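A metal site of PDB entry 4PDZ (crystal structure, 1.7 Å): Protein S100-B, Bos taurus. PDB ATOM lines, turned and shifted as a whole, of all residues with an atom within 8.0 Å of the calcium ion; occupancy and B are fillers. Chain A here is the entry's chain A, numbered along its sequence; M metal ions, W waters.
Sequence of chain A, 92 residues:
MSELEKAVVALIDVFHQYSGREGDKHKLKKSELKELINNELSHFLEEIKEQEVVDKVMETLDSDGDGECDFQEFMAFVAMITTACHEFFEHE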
ATOM      1  N   LYS A  27     -23.858 -16.078  27.542  1.00  0.00           N
ATOM      2  CA  LYS A  27     -23.685 -16.102  26.086  1.00  0.00           C
ATOM      3  C   LYS A  27     -24.877 -16.777  25.401  1.00  0.00           C
ATOM      4  O   LYS A  27     -25.618 -17.518  26.026  1.00  0.00           O
ATOM      5  CB  LYS A  27     -22.374 -16.816  25.717  1.00  0.00           C
ATOM      6  CG  LYS A  27     -21.103 -16.068  26.173  1.00  0.00           C
ATOM      7  CD  LYS A  27     -19.834 -16.712  25.596  1.00  0.00           C
ATOM      8  CE  LYS A  27     -18.582 -16.293  26.367  1.00  0.00           C
ATOM      9  NZ  LYS A  27     -18.695 -16.623  27.826  1.00  0.00           N
ATOM     10  N   LEU A  28     -25.055 -16.478  24.117  1.00  0.00           N
ATOM     11  CA  LEU A  28     -26.138 -17.061  23.328  1.00  0.00           C
ATOM     12  C   LEU A  28     -25.599 -18.162  22.459  1.00  0.00           C
ATOM     13  O   LEU A  28     -24.808 -17.891  21.546  1.00  0.00           O
ATOM     14  CB  LEU A  28     -26.758 -16.014  22.409  1.00  0.00           C
ATOM     15  CG  LEU A  28     -27.400 -14.795  23.041  1.00  0.00           C
ATOM     16  CD1 LEU A  28     -27.625 -13.736  21.945  1.00  0.00           C
ATOM     17  CD2 LEU A  28     -28.692 -15.164  23.728  1.00  0.00           C
ATOM     18  N   MET A  58     -24.912 -16.924  13.168  1.00  0.00           N
ATOM     19  CA  MET A  58     -23.890 -17.034  14.212  1.00  0.00           C
ATOM     20  C   MET A  58     -22.458 -16.831  13.703  1.00  0.00           C
ATOM     21  O   MET A  58     -21.658 -16.196  14.391  1.00  0.00           O
ATOM     22  CB  MET A  58     -23.994 -18.383  14.944  1.00  0.00           C
ATOM     23  CG  MET A  58     -22.965 -18.526  16.042  1.00  0.00           C
ATOM     24  SD  MET A  58     -23.325 -17.478  17.479  1.00  0.00           S
ATOM     25  CE  MET A  58     -24.622 -18.436  18.263  1.00  0.00           C
ATOM     26  N   LEU A  61     -21.948 -13.078  13.433  1.00  0.00           N
ATOM     27  CA  LEU A  61     -21.885 -12.334  14.688  1.00  0.00           C
ATOM     28  C   LEU A  61     -20.737 -12.745  15.615  1.00  0.00           C
ATOM     29  O   LEU A  61     -20.282 -11.934  16.423  1.00  0.00           O
ATOM     30  CB  LEU A  61     -23.222 -12.469  15.443  1.00  0.00           C
ATOM     31  CG  LEU A  61     -24.503 -12.080  14.703  1.00  0.00           C
ATOM     32  CD1 LEU A  61     -25.735 -12.253  15.596  1.00  0.00           C
ATOM     33  CD2 LEU A  61     -24.413 -10.641  14.209  1.00  0.00           C
ATOM     34  N   ASP A  62     -20.262 -13.976  15.515  1.00  0.00           N
ATOM     35  CA  ASP A  62     -19.243 -14.401  16.475  1.00  0.00           C
ATOM     36  C   ASP A  62     -17.807 -13.988  16.109  1.00  0.00           C
ATOM     37  O   ASP A  62     -17.070 -14.733  15.449  1.00  0.00           O
ATOM     38  CB  ASP A  62     -19.327 -15.899  16.786  1.00  0.00           C
ATOM     39  CG  ASP A  62     -18.475 -16.267  17.988  1.00  0.00           C
ATOM     40  OD1 ASP A  62     -18.162 -15.367  18.795  1.00  0.00           O
ATOM     41  OD2 ASP A  62     -18.186 -17.441  18.193  1.00  0.00           O
ATOM     42  N   SER A  63     -17.446 -12.796  16.549  1.00  0.00           N
ATOM     43  CA  SER A  63     -16.151 -12.202  16.240  1.00  0.00           C
ATOM     44  C   SER A  63     -14.976 -12.882  16.930  1.00  0.00           C
ATOM     45  O   SER A  63     -13.864 -12.863  16.403  1.00  0.00           O
ATOM     46  CB  SER A  63     -16.159 -10.716  16.598  1.00  0.00           C
ATOM     47  OG  SER A  63     -16.745  -9.945  15.570  1.00  0.00           O
ATOM     48  N   ASP A  64     -15.209 -13.493  18.085  1.00  0.00           N
ATOM     49  CA  ASP A  64     -14.100 -14.105  18.807  1.00  0.00           C
ATOM     50  C   ASP A  64     -13.932 -15.561  18.409  1.00  0.00           C
ATOM     51  O   ASP A  64     -12.817 -16.106  18.421  1.00  0.00           O
ATOM     52  CB  ASP A  64     -14.172 -13.896  20.330  1.00  0.00           C
ATOM     53  CG  ASP A  64     -15.400 -14.528  20.978  1.00  0.00           C
ATOM     54  OD1 ASP A  64     -16.029 -15.433  20.385  1.00  0.00           O
ATOM     55  OD2 ASP A  64     -15.723 -14.124  22.119  1.00  0.00           O
ATOM     56  N   GLY A  65     -15.038 -16.218  18.070  1.00  0.00           N
ATOM     57  CA  GLY A  65     -14.955 -17.552  17.505  1.00  0.00           C
ATOM     58  C   GLY A  65     -15.354 -18.712  18.397  1.00  0.00           C
ATOM     59  O   GLY A  65     -15.227 -19.865  17.975  1.00  0.00           O
ATOM     60  N   ASP A  66     -15.814 -18.440  19.608  1.00  0.00           N
ATOM     61  CA  ASP A  66     -16.177 -19.521  20.541  1.00  0.00           C
ATOM     62  C   ASP A  66     -17.507 -20.212  20.221  1.00  0.00           C
ATOM     63  O   ASP A  66     -18.019 -21.000  21.024  1.00  0.00           O
ATOM     64  CB  ASP A  66     -16.114 -19.056  22.006  1.00  0.00           C
ATOM     65  CG  ASP A  66     -17.050 -17.895  22.324  1.00  0.00           C
ATOM     66  OD1 ASP A  66     -17.941 -17.595  21.502  1.00  0.00           O
ATOM     67  OD2 ASP A  66     -16.897 -17.289  23.408  1.00  0.00           O
ATOM     68  N   GLY A  67     -18.071 -19.904  19.050  1.00  0.00           N
ATOM     69  CA  GLY A  67     -19.299 -20.534  18.588  1.00  0.00           C
ATOM     70  C   GLY A  67     -20.581 -19.995  19.185  1.00  0.00           C
ATOM     71  O   GLY A  67     -21.668 -20.447  18.839  1.00  0.00           O
ATOM     72  N   GLU A  68     -20.454 -19.013  20.073  1.00  0.00           N
ATOM     73  CA  GLU A  68     -21.618 -18.378  20.696  1.00  0.00           C
ATOM     74  C   GLU A  68     -21.536 -16.870  20.543  1.00  0.00           C
ATOM     75  O   GLU A  68     -20.543 -16.346  20.041  1.00  0.00           O
ATOM     76  CB  GLU A  68     -21.718 -18.718  22.192  1.00  0.00           C
ATOM     77  CG  GLU A  68     -21.508 -20.182  22.524  1.00  0.00           C
ATOM     78  CD  GLU A  68     -22.362 -20.639  23.708  1.00  0.00           C
ATOM     79  OE1 GLU A  68     -22.966 -19.770  24.396  1.00  0.00           O
ATOM     80  OE2 GLU A  68     -22.465 -21.865  23.922  1.00  0.00           O
ATOM     81  N   CYS A  69     -22.619 -16.186  20.897  1.00  0.00           N
ATOM     82  CA  CYS A  69     -22.690 -14.734  20.807  1.00  0.00           C
ATOM     83  C   CYS A  69     -22.712 -14.127  22.210  1.00  0.00           C
ATOM     84  O   CYS A  69     -23.710 -14.299  22.929  1.00  0.00           O
ATOM     85  CB  CYS A  69     -23.933 -14.311  20.017  1.00  0.00           C
ATOM     86  SG  CYS A  69     -24.155 -12.511  19.835  1.00  0.00           S
ATOM     87  N   ASP A  70     -21.635 -13.455  22.607  1.00  0.00           N
ATOM     88  CA  ASP A  70     -21.572 -12.782  23.908  1.00  0.00           C
ATOM     89  C   ASP A  70     -22.250 -11.412  23.867  1.00  0.00           C
ATOM     90  O   ASP A  70     -22.661 -10.966  22.798  1.00  0.00           O
ATOM     91  CB  ASP A  70     -20.130 -12.686  24.456  1.00  0.00           C
ATOM     92  CG  ASP A  70     -19.206 -11.837  23.583  1.00  0.00           C
ATOM     93  OD1 ASP A  70     -19.681 -10.955  22.830  1.00  0.00           O
ATOM     94  OD2 ASP A  70     -17.967 -12.044  23.651  1.00  0.00           O
ATOM     95  N   PHE A  71     -22.305 -10.713  24.999  1.00  0.00           N
ATOM     96  CA  PHE A  71     -23.040  -9.446  25.007  1.00  0.00           C
ATOM     97  C   PHE A  71     -22.470  -8.418  24.038  1.00  0.00           C
ATOM     98  O   PHE A  71     -23.211  -7.660  23.383  1.00  0.00           O
ATOM     99  CB  PHE A  71     -23.126  -8.837  26.412  1.00  0.00           C
ATOM    100  CG  PHE A  71     -23.952  -7.593  26.469  1.00  0.00           C
ATOM    101  CD1 PHE A  71     -25.338  -7.662  26.513  1.00  0.00           C
ATOM    102  CD2 PHE A  71     -23.350  -6.343  26.439  1.00  0.00           C
ATOM    103  CE1 PHE A  71     -26.109  -6.495  26.539  1.00  0.00           C
ATOM    104  CE2 PHE A  71     -24.105  -5.182  26.480  1.00  0.00           C
ATOM    105  CZ  PHE A  71     -25.493  -5.260  26.522  1.00  0.00           C
ATOM    106  N   GLN A  72     -21.148  -8.397  23.928  1.00  0.00           N
ATOM    107  CA  GLN A  72     -20.446  -7.425  23.115  1.00  0.00           C
ATOM    108  C   GLN A  72     -20.702  -7.682  21.624  1.00  0.00           C
ATOM    109  O   GLN A  72     -20.791  -6.748  20.819  1.00  0.00           O
ATOM    110  CB  GLN A  72     -18.963  -7.461  23.503  1.00  0.00           C
ATOM    111  CG  GLN A  72     -18.078  -8.390  22.694  1.00  0.00           C
ATOM    112  CD  GLN A  72     -16.638  -8.452  23.200  1.00  0.00           C
ATOM    113  OE1 GLN A  72     -15.984  -7.421  23.389  1.00  0.00           O
ATOM    114  NE2 GLN A  72     -16.155  -9.670  23.442  1.00  0.00           N
ATOM    115  N   GLU A  73     -20.838  -8.946  21.279  1.00  0.00           N
ATOM    116  CA  GLU A  73     -21.174  -9.339  19.924  1.00  0.00           C
ATOM    117  C   GLU A  73     -22.656  -9.064  19.634  1.00  0.00           C
ATOM    118  O   GLU A  73     -23.040  -8.735  18.501  1.00  0.00           O
ATOM    119  CB  GLU A  73     -20.797 -10.807  19.698  1.00  0.00           C
ATOM    120  CG  GLU A  73     -19.288 -10.989  19.596  1.00  0.00           C
ATOM    121  CD  GLU A  73     -18.826 -12.432  19.686  1.00  0.00           C
ATOM    122  OE1 GLU A  73     -19.601 -13.284  20.174  1.00  0.00           O
ATOM    123  OE2 GLU A  73     -17.677 -12.703  19.276  1.00  0.00           O
HETATM  124 CA    CA M   1     -18.407 -15.464  20.565  1.00  0.00          CA
HETATM  125  O   HOH W   1     -18.221 -14.688  22.903  1.00  0.00           O
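Of the 16 residues printed, 5 come within 4 Å of the calcium ion.
The calcium ion is bound by OD1 of Asp 62 (1.8 Å), O of Glu 68 (2.4 Å), OD1 of Asp 66 (2.4 Å), OD1 of Asp 64 (2.4 Å), water W1 (2.5 Å) and OE1 of Glu 73 (2.5 Å). The calcium ion has six donor atoms within binding distance. Slightly farther from the calcium ion lies OD2 of Asp 62 (3.1 Å). Slightly farther from the calcium ion lies OE2 of Glu 73 (3.1 Å).
N of Ser 63 sits at hydrogen-bond distance from OE2 of Glu 73, 2.7 Å away. N of Gly 65 lies close to OD2 of Asp 62, at 3.4 Å. The backbone NH (N) of Glu 73 sits at hydrogen-bond distance from the side-chain carboxylate (OD1) of Asp 70. The side-chain carboxylate (OD2) of Asp 62 lies within hydrogen-bond range of the backbone NH (N) of Gly 67, 2.6 Å away.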
